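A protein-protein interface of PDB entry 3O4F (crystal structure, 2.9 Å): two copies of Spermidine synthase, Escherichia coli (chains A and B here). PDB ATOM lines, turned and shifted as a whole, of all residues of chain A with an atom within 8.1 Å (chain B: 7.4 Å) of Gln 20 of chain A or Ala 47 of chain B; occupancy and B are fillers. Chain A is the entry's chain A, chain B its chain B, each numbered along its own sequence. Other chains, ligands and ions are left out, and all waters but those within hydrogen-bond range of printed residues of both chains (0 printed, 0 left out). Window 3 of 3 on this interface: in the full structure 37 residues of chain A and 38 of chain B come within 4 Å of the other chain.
O of Ala 26 of chain B lies within hydrogen-bond range of ND2 of Asn 46 of chain B, 3.0 Å away.
N of Ala 47 of chain B lies within hydrogen-bond range of OD2 of Asp 28 of chain B, at 2.9 Å.
The side-chain amide oxygen of Asn 46 of chain B lies within hydrogen-bond range of the backbone NH of Ala 48 of chain B.
OD1 of Asn 46 of chain B is in hydrogen-bond range of N of Phe 49 of chain B (2.8 Å).
Among the printed residues, merely in contact across the chains: Gln 20 of chain A with Phe 25 of chain B, Gln 20 of chain A with Ala 47 of chain B, Phe 21 of chain A with Tyr 24 of chain B, Phe 21 of chain A with Phe 25 of chain B and Phe 21 of chain A with Ala 48 of chain B.
Printed residues of chain B that touch a printed residue of chain A: Tyr 24, Phe 25, Ala 26, Asn 46, Ala 47 and Ala 48.
Hydrophobic or aromatic side chains of chain B that line the printed part of chain A: Tyr 24, Phe 25, Ala 26, Ala 47 and Ala 48.
Gln 20 of chain A touches just these residues of chain B: Phe 25 (3.5 Å), Ala 26 (2.6 Å), Asn 46 (3.0 Å) and Ala 47 (3.6 Å).
Of chain A, only Gln 20 (3.0 Å) comes within 4 Å of Asn 46 of chain B.
Of chain A, only Phe 21 (3.5 Å) comes within 4 Å of Ala 48 of chain B.
Of the printed residues of chain A, Phe 25 of chain B touches Gln 20 and Phe 21.
Of the printed residues of chain A, Ala 26 of chain B touches Gln 20 (2.6 Å).
Of the printed residues of chain B, Phe 21 of chain A touches Tyr 24 (3.3 Å), Phe 25 (3.97 Å) and Ala 48 (3.5 Å).
Gln 12 of chain B touches none of the printed residues of chain A.
The nearest residue of chain B that does not touch Gln 20 of chain A is Asp 28 of chain B (4.1 Å).
The nearest residue of chain A that does not touch Ala 47 of chain B is Phe 21 of chain A (6.6 Å).
No position is printed for both chains.
Of the 9 pairs that touch across the chains among the printed residues, none has its exchanged pair printed and touching as well.
The side-chain hydroxyl (OH) of Tyr 24 of chain B sits at hydrogen-bond distance from the backbone carbonyl oxygen (O) of Glu 15 of chain A.
The backbone carbonyl oxygen (O) of Gln 20 of chain A is in hydrogen-bond range of the backbone NH (N) of Ala 26 of chain B, 2.6 Å away.
The backbone carbonyl oxygen (O) of Gln 20 of chain A is in hydrogen-bond range of the side-chain amide nitrogen (ND2) of Asn 46 of chain B, at 3.0 Å.
N of Tyr 24 of chain B is in hydrogen-bond range of O of Gly 22 of chain A (2.8 Å).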
ATOM      1  N   GLU A  15     -36.854  -6.611 -14.422  1.00  0.00           N
ATOM      2  CA  GLU A  15     -37.735  -5.607 -14.973  1.00  0.00           C
ATOM      3  C   GLU A  15     -37.737  -5.813 -16.474  1.00  0.00           C
ATOM      4  O   GLU A  15     -36.728  -6.188 -17.034  1.00  0.00           O
ATOM      5  CB  GLU A  15     -37.268  -4.208 -14.610  1.00  0.00           C
ATOM      6  CG  GLU A  15     -38.339  -3.165 -14.859  1.00  0.00           C
ATOM      7  CD  GLU A  15     -37.872  -1.743 -14.590  1.00  0.00           C
ATOM      8  OE1 GLU A  15     -36.692  -1.435 -14.915  1.00  0.00           O
ATOM      9  OE2 GLU A  15     -38.685  -0.934 -14.078  1.00  0.00           O
ATOM     10  N   THR A  16     -38.869  -5.567 -17.119  1.00  0.00           N
ATOM     11  CA  THR A  16     -39.002  -5.717 -18.571  1.00  0.00           C
ATOM     12  C   THR A  16     -39.287  -4.400 -19.312  1.00  0.00           C
ATOM     13  O   THR A  16     -39.566  -4.404 -20.513  1.00  0.00           O
ATOM     14  CB  THR A  16     -40.113  -6.654 -18.845  1.00  0.00           C
ATOM     15  OG1 THR A  16     -39.920  -7.762 -17.992  1.00  0.00           O
ATOM     16  CG2 THR A  16     -40.091  -7.119 -20.288  1.00  0.00           C
ATOM     17  N   LEU A  17     -39.184  -3.278 -18.612  1.00  0.00           N
ATOM     18  CA  LEU A  17     -39.626  -2.032 -19.167  1.00  0.00           C
ATOM     19  C   LEU A  17     -38.949  -1.821 -20.510  1.00  0.00           C
ATOM     20  O   LEU A  17     -39.633  -1.424 -21.454  1.00  0.00           O
ATOM     21  CB  LEU A  17     -39.317  -0.873 -18.219  1.00  0.00           C
ATOM     22  CG  LEU A  17     -39.671   0.542 -18.720  1.00  0.00           C
ATOM     23  CD1 LEU A  17     -41.004   0.532 -19.445  1.00  0.00           C
ATOM     24  CD2 LEU A  17     -39.647   1.550 -17.590  1.00  0.00           C
ATOM     25  N   HIS A  18     -37.633  -2.081 -20.587  1.00  0.00           N
ATOM     26  CA  HIS A  18     -36.898  -2.032 -21.863  1.00  0.00           C
ATOM     27  C   HIS A  18     -36.407  -3.439 -22.285  1.00  0.00           C
ATOM     28  O   HIS A  18     -36.072  -4.302 -21.443  1.00  0.00           O
ATOM     29  CB  HIS A  18     -35.732  -1.027 -21.804  1.00  0.00           C
ATOM     30  CG  HIS A  18     -36.129   0.313 -21.283  1.00  0.00           C
ATOM     31  ND1 HIS A  18     -35.721   0.768 -20.049  1.00  0.00           N
ATOM     32  CD2 HIS A  18     -36.921   1.278 -21.797  1.00  0.00           C
ATOM     33  CE1 HIS A  18     -36.238   1.960 -19.826  1.00  0.00           C
ATOM     34  NE2 HIS A  18     -36.972   2.291 -20.873  1.00  0.00           N
ATOM     35  N   ASP A  19     -36.373  -3.669 -23.593  1.00  0.00           N
ATOM     36  CA  ASP A  19     -35.922  -4.946 -24.131  1.00  0.00           C
ATOM     37  C   ASP A  19     -34.413  -5.136 -24.025  1.00  0.00           C
ATOM     38  O   ASP A  19     -33.937  -6.248 -23.851  1.00  0.00           O
ATOM     39  CB  ASP A  19     -36.359  -5.093 -25.590  1.00  0.00           C
ATOM     40  CG  ASP A  19     -37.855  -5.309 -25.733  1.00  0.00           C
ATOM     41  OD1 ASP A  19     -38.630  -4.593 -25.057  1.00  0.00           O
ATOM     42  OD2 ASP A  19     -38.264  -6.181 -26.522  1.00  0.00           O
ATOM     43  N   GLN A  20     -33.667  -4.043 -24.105  1.00  0.00           N
ATOM     44  CA  GLN A  20     -32.230  -4.100 -24.264  1.00  0.00           C
ATOM     45  C   GLN A  20     -31.440  -4.155 -22.976  1.00  0.00           C
ATOM     46  O   GLN A  20     -30.275  -4.535 -22.991  1.00  0.00           O
ATOM     47  CB  GLN A  20     -31.782  -2.880 -25.073  1.00  0.00           C
ATOM     48  CG  GLN A  20     -32.210  -2.947 -26.535  1.00  0.00           C
ATOM     49  CD  GLN A  20     -31.950  -4.294 -27.146  1.00  0.00           C
ATOM     50  OE1 GLN A  20     -30.799  -4.753 -27.193  1.00  0.00           O
ATOM     51  NE2 GLN A  20     -33.000  -4.934 -27.628  1.00  0.00           N
ATOM     52  N   PHE A  21     -32.047  -3.762 -21.871  1.00  0.00           N
ATOM     53  CA  PHE A  21     -31.353  -3.706 -20.600  1.00  0.00           C
ATOM     54  C   PHE A  21     -32.351  -3.531 -19.482  1.00  0.00           C
ATOM     55  O   PHE A  21     -33.486  -3.137 -19.718  1.00  0.00           O
ATOM     56  CB  PHE A  21     -30.458  -2.506 -20.584  1.00  0.00           C
ATOM     57  CG  PHE A  21     -31.215  -1.248 -20.728  1.00  0.00           C
ATOM     58  CD1 PHE A  21     -31.570  -0.784 -21.983  1.00  0.00           C
ATOM     59  CD2 PHE A  21     -31.661  -0.573 -19.616  1.00  0.00           C
ATOM     60  CE1 PHE A  21     -32.319   0.362 -22.127  1.00  0.00           C
ATOM     61  CE2 PHE A  21     -32.437   0.584 -19.747  1.00  0.00           C
ATOM     62  CZ  PHE A  21     -32.766   1.049 -21.000  1.00  0.00           C
ATOM     63  N   GLY A  22     -31.954  -3.792 -18.249  1.00  0.00           N
ATOM     64  CA  GLY A  22     -32.880  -3.565 -17.136  1.00  0.00           C
ATOM     65  C   GLY A  22     -32.208  -3.656 -15.802  1.00  0.00           C
ATOM     66  O   GLY A  22     -30.981  -3.724 -15.715  1.00  0.00           O
ATOM     67  N   LEU A 203     -31.990   8.243 -21.834  1.00  0.00           N
ATOM     68  CA  LEU A 203     -32.237   7.565 -23.091  1.00  0.00           C
ATOM     69  C   LEU A 203     -32.981   8.312 -24.156  1.00  0.00           C
ATOM     70  O   LEU A 203     -32.775   8.107 -25.317  1.00  0.00           O
ATOM     71  CB  LEU A 203     -32.929   6.258 -22.837  1.00  0.00           C
ATOM     72  CG  LEU A 203     -32.009   5.117 -22.483  1.00  0.00           C
ATOM     73  CD1 LEU A 203     -30.924   5.079 -23.452  1.00  0.00           C
ATOM     74  CD2 LEU A 203     -31.461   5.315 -21.127  1.00  0.00           C
ATOM     75  N   LYS B  11     -28.969 -13.592 -25.667  1.00  0.00           N
ATOM     76  CA  LYS B  11     -27.817 -13.528 -24.726  1.00  0.00           C
ATOM     77  C   LYS B  11     -27.898 -12.241 -23.895  1.00  0.00           C
ATOM     78  O   LYS B  11     -28.145 -11.175 -24.440  1.00  0.00           O
ATOM     79  CB  LYS B  11     -26.492 -13.583 -25.491  1.00  0.00           C
ATOM     80  CG  LYS B  11     -25.345 -14.210 -24.691  1.00  0.00           C
ATOM     81  CD  LYS B  11     -24.064 -14.403 -25.545  1.00  0.00           C
ATOM     82  CE  LYS B  11     -23.197 -15.559 -25.037  1.00  0.00           C
ATOM     83  NZ  LYS B  11     -23.950 -16.859 -25.017  1.00  0.00           N
ATOM     84  N   GLN B  12     -27.702 -12.345 -22.580  1.00  0.00           N
ATOM     85  CA  GLN B  12     -27.682 -11.184 -21.676  1.00  0.00           C
ATOM     86  C   GLN B  12     -26.467 -11.224 -20.763  1.00  0.00           C
ATOM     87  O   GLN B  12     -25.709 -12.197 -20.745  1.00  0.00           O
ATOM     88  CB  GLN B  12     -28.940 -11.146 -20.827  1.00  0.00           C
ATOM     89  CG  GLN B  12     -30.215 -11.198 -21.631  1.00  0.00           C
ATOM     90  CD  GLN B  12     -31.369 -10.590 -20.879  1.00  0.00           C
ATOM     91  OE1 GLN B  12     -31.932  -9.537 -21.281  1.00  0.00           O
ATOM     92  NE2 GLN B  12     -31.728 -11.235 -19.755  1.00  0.00           N
ATOM     93  N   TYR B  24     -28.651  -5.300 -15.771  1.00  0.00           N
ATOM     94  CA  TYR B  24     -28.248  -6.224 -16.818  1.00  0.00           C
ATOM     95  C   TYR B  24     -28.414  -5.591 -18.189  1.00  0.00           C
ATOM     96  O   TYR B  24     -29.114  -4.581 -18.317  1.00  0.00           O
ATOM     97  CB  TYR B  24     -29.070  -7.494 -16.739  1.00  0.00           C
ATOM     98  CG  TYR B  24     -30.505  -7.308 -17.153  1.00  0.00           C
ATOM     99  CD1 TYR B  24     -31.480  -6.954 -16.232  1.00  0.00           C
ATOM    100  CD2 TYR B  24     -30.893  -7.485 -18.467  1.00  0.00           C
ATOM    101  CE1 TYR B  24     -32.817  -6.787 -16.611  1.00  0.00           C
ATOM    102  CE2 TYR B  24     -32.227  -7.331 -18.855  1.00  0.00           C
ATOM    103  CZ  TYR B  24     -33.186  -6.975 -17.923  1.00  0.00           C
ATOM    104  OH  TYR B  24     -34.497  -6.778 -18.322  1.00  0.00           O
ATOM    105  N   PHE B  25     -27.765  -6.188 -19.197  1.00  0.00           N
ATOM    106  CA  PHE B  25     -27.792  -5.665 -20.563  1.00  0.00           C
ATOM    107  C   PHE B  25     -27.930  -6.775 -21.573  1.00  0.00           C
ATOM    108  O   PHE B  25     -27.347  -7.832 -21.401  1.00  0.00           O
ATOM    109  CB  PHE B  25     -26.498  -4.906 -20.903  1.00  0.00           C
ATOM    110  CG  PHE B  25     -26.118  -3.881 -19.900  1.00  0.00           C
ATOM    111  CD1 PHE B  25     -26.528  -2.585 -20.032  1.00  0.00           C
ATOM    112  CD2 PHE B  25     -25.363  -4.221 -18.810  1.00  0.00           C
ATOM    113  CE1 PHE B  25     -26.183  -1.645 -19.111  1.00  0.00           C
ATOM    114  CE2 PHE B  25     -25.006  -3.273 -17.884  1.00  0.00           C
ATOM    115  CZ  PHE B  25     -25.420  -1.990 -18.037  1.00  0.00           C
ATOM    116  N   ALA B  26     -28.663  -6.497 -22.660  1.00  0.00           N
ATOM    117  CA  ALA B  26     -28.662  -7.368 -23.842  1.00  0.00           C
ATOM    118  C   ALA B  26     -27.281  -7.253 -24.459  1.00  0.00           C
ATOM    119  O   ALA B  26     -26.681  -6.188 -24.435  1.00  0.00           O
ATOM    120  CB  ALA B  26     -29.719  -6.949 -24.835  1.00  0.00           C
ATOM    121  N   VAL B  27     -26.768  -8.361 -24.979  1.00  0.00           N
ATOM    122  CA  VAL B  27     -25.536  -8.349 -25.734  1.00  0.00           C
ATOM    123  C   VAL B  27     -25.854  -8.501 -27.211  1.00  0.00           C
ATOM    124  O   VAL B  27     -26.435  -9.490 -27.616  1.00  0.00           O
ATOM    125  CB  VAL B  27     -24.620  -9.478 -25.299  1.00  0.00           C
ATOM    126  CG1 VAL B  27     -23.361  -9.475 -26.161  1.00  0.00           C
ATOM    127  CG2 VAL B  27     -24.272  -9.322 -23.850  1.00  0.00           C
ATOM    128  N   ASP B  28     -25.478  -7.515 -28.012  1.00  0.00           N
ATOM    129  CA  ASP B  28     -25.621  -7.624 -29.444  1.00  0.00           C
ATOM    130  C   ASP B  28     -24.410  -8.375 -30.032  1.00  0.00           C
ATOM    131  O   ASP B  28     -24.536  -9.106 -31.023  1.00  0.00           O
ATOM    132  CB  ASP B  28     -25.809  -6.234 -30.049  1.00  0.00           C
ATOM    133  CG  ASP B  28     -27.149  -5.630 -29.673  1.00  0.00           C
ATOM    134  OD1 ASP B  28     -28.162  -6.335 -29.836  1.00  0.00           O
ATOM    135  OD2 ASP B  28     -27.222  -4.465 -29.208  1.00  0.00           O
ATOM    136  N   PHE B  44     -18.451  -5.654 -24.676  1.00  0.00           N
ATOM    137  CA  PHE B  44     -19.499  -6.006 -25.614  1.00  0.00           C
ATOM    138  C   PHE B  44     -20.369  -4.827 -25.960  1.00  0.00           C
ATOM    139  O   PHE B  44     -20.401  -3.843 -25.217  1.00  0.00           O
ATOM    140  CB  PHE B  44     -20.364  -7.064 -25.012  1.00  0.00           C
ATOM    141  CG  PHE B  44     -21.093  -6.625 -23.794  1.00  0.00           C
ATOM    142  CD1 PHE B  44     -20.531  -6.749 -22.556  1.00  0.00           C
ATOM    143  CD2 PHE B  44     -22.359  -6.112 -23.893  1.00  0.00           C
ATOM    144  CE1 PHE B  44     -21.224  -6.359 -21.412  1.00  0.00           C
ATOM    145  CE2 PHE B  44     -23.056  -5.708 -22.756  1.00  0.00           C
ATOM    146  CZ  PHE B  44     -22.479  -5.842 -21.510  1.00  0.00           C
ATOM    147  N   GLU B  45     -21.067  -4.936 -27.093  1.00  0.00           N
ATOM    148  CA  GLU B  45     -21.908  -3.839 -27.584  1.00  0.00           C
ATOM    149  C   GLU B  45     -23.310  -4.119 -27.105  1.00  0.00           C
ATOM    150  O   GLU B  45     -23.768  -5.258 -27.156  1.00  0.00           O
ATOM    151  CB  GLU B  45     -21.877  -3.696 -29.122  1.00  0.00           C
ATOM    152  CG  GLU B  45     -20.507  -3.949 -29.754  1.00  0.00           C
ATOM    153  CD  GLU B  45     -20.264  -3.117 -31.001  1.00  0.00           C
ATOM    154  OE1 GLU B  45     -20.236  -1.869 -30.864  1.00  0.00           O
ATOM    155  OE2 GLU B  45     -20.067  -3.713 -32.093  1.00  0.00           O
ATOM    156  N   ASN B  46     -23.964  -3.063 -26.641  1.00  0.00           N
ATOM    157  CA  ASN B  46     -25.351  -3.091 -26.242  1.00  0.00           C
ATOM    158  C   ASN B  46     -26.072  -1.932 -26.950  1.00  0.00           C
ATOM    159  O   ASN B  46     -25.534  -0.825 -27.023  1.00  0.00           O
ATOM    160  CB  ASN B  46     -25.438  -2.916 -24.737  1.00  0.00           C
ATOM    161  CG  ASN B  46     -26.807  -2.474 -24.283  1.00  0.00           C
ATOM    162  OD1 ASN B  46     -27.072  -1.272 -24.096  1.00  0.00           O
ATOM    163  ND2 ASN B  46     -27.691  -3.434 -24.112  1.00  0.00           N
ATOM    164  N   ALA B  47     -27.284  -2.181 -27.439  1.00  0.00           N
ATOM    165  CA  ALA B  47     -28.050  -1.166 -28.197  1.00  0.00           C
ATOM    166  C   ALA B  47     -28.167   0.206 -27.507  1.00  0.00           C
ATOM    167  O   ALA B  47     -28.127   1.247 -28.143  1.00  0.00           O
ATOM    168  CB  ALA B  47     -29.476  -1.708 -28.511  1.00  0.00           C
ATOM    169  N   ALA B  48     -28.345   0.177 -26.197  1.00  0.00           N
ATOM    170  CA  ALA B  48     -28.671   1.356 -25.430  1.00  0.00           C
ATOM    171  C   ALA B  48     -27.440   2.129 -25.061  1.00  0.00           C
ATOM    172  O   ALA B  48     -27.388   3.370 -25.274  1.00  0.00           O
ATOM    173  CB  ALA B  48     -29.423   0.965 -24.161  1.00  0.00           C
ATOM    174  N   PHE B  49     -26.454   1.420 -24.502  1.00  0.00           N
ATOM    175  CA  PHE B  49     -25.281   2.085 -23.933  1.00  0.00           C
ATOM    176  C   PHE B  49     -23.969   1.901 -24.719  1.00  0.00           C
ATOM    177  O   PHE B  49     -22.876   2.231 -24.231  1.00  0.00           O
ATOM    178  CB  PHE B  49     -25.092   1.588 -22.533  1.00  0.00           C
ATOM    179  CG  PHE B  49     -26.184   1.973 -21.619  1.00  0.00           C
ATOM    180  CD1 PHE B  49     -26.243   3.251 -21.101  1.00  0.00           C
ATOM    181  CD2 PHE B  49     -27.153   1.058 -21.254  1.00  0.00           C
ATOM    182  CE1 PHE B  49     -27.234   3.620 -20.235  1.00  0.00           C
ATOM    183  CE2 PHE B  49     -28.149   1.414 -20.389  1.00  0.00           C
ATOM    184  CZ  PHE B  49     -28.185   2.703 -19.881  1.00  0.00           C
ATOM    185  N   GLY B  50     -24.084   1.371 -25.935  1.00  0.00           N
ATOM    186  CA  GLY B  50     -22.933   1.165 -26.792  1.00  0.00           C
ATOM    187  C   GLY B  50     -21.973   0.175 -26.186  1.00  0.00           C
ATOM    188  O   GLY B  50     -22.399  -0.791 -25.575  1.00  0.00           O
ATOM    189  N   ARG B  51     -20.678   0.442 -26.330  1.00  0.00           N
ATOM    190  CA  ARG B  51     -19.665  -0.459 -25.807  1.00  0.00           C
ATOM    191  C   ARG B  51     -19.603  -0.420 -24.286  1.00  0.00           C
ATOM    192  O   ARG B  51     -19.573   0.638 -23.698  1.00  0.00           O
ATOM    193  CB  ARG B  51     -18.297  -0.120 -26.392  1.00  0.00           C
ATOM    194  CG  ARG B  51     -18.122  -0.565 -27.848  1.00  0.00           C
ATOM    195  CD  ARG B  51     -17.010   0.203 -28.499  1.00  0.00           C
ATOM    196  NE  ARG B  51     -16.071  -0.677 -29.189  1.00  0.00           N
ATOM    197  CZ  ARG B  51     -15.937  -0.779 -30.499  1.00  0.00           C
ATOM    198  NH1 ARG B  51     -16.673  -0.064 -31.344  1.00  0.00           N
ATOM    199  NH2 ARG B  51     -15.051  -1.623 -30.967  1.00  0.00           N
ATOM    200  N   ARG B  64     -21.836   5.204 -23.995  1.00  0.00           N
ATOM    201  CA  ARG B  64     -22.889   6.197 -24.139  1.00  0.00           C
ATOM    202  C   ARG B  64     -23.073   7.177 -22.965  1.00  0.00           C
ATOM    203  O   ARG B  64     -23.615   8.279 -23.170  1.00  0.00           O
ATOM    204  CB  ARG B  64     -24.203   5.479 -24.400  1.00  0.00           C
ATOM    205  CG  ARG B  64     -25.276   6.320 -25.031  1.00  0.00           C
ATOM    206  CD  ARG B  64     -24.996   6.578 -26.500  1.00  0.00           C
ATOM    207  NE  ARG B  64     -25.010   5.328 -27.266  1.00  0.00           N
ATOM    208  CZ  ARG B  64     -24.087   4.967 -28.155  1.00  0.00           C
ATOM    209  NH1 ARG B  64     -24.223   3.817 -28.807  1.00  0.00           N
ATOM    210  NH2 ARG B  64     -23.052   5.763 -28.420  1.00  0.00           N
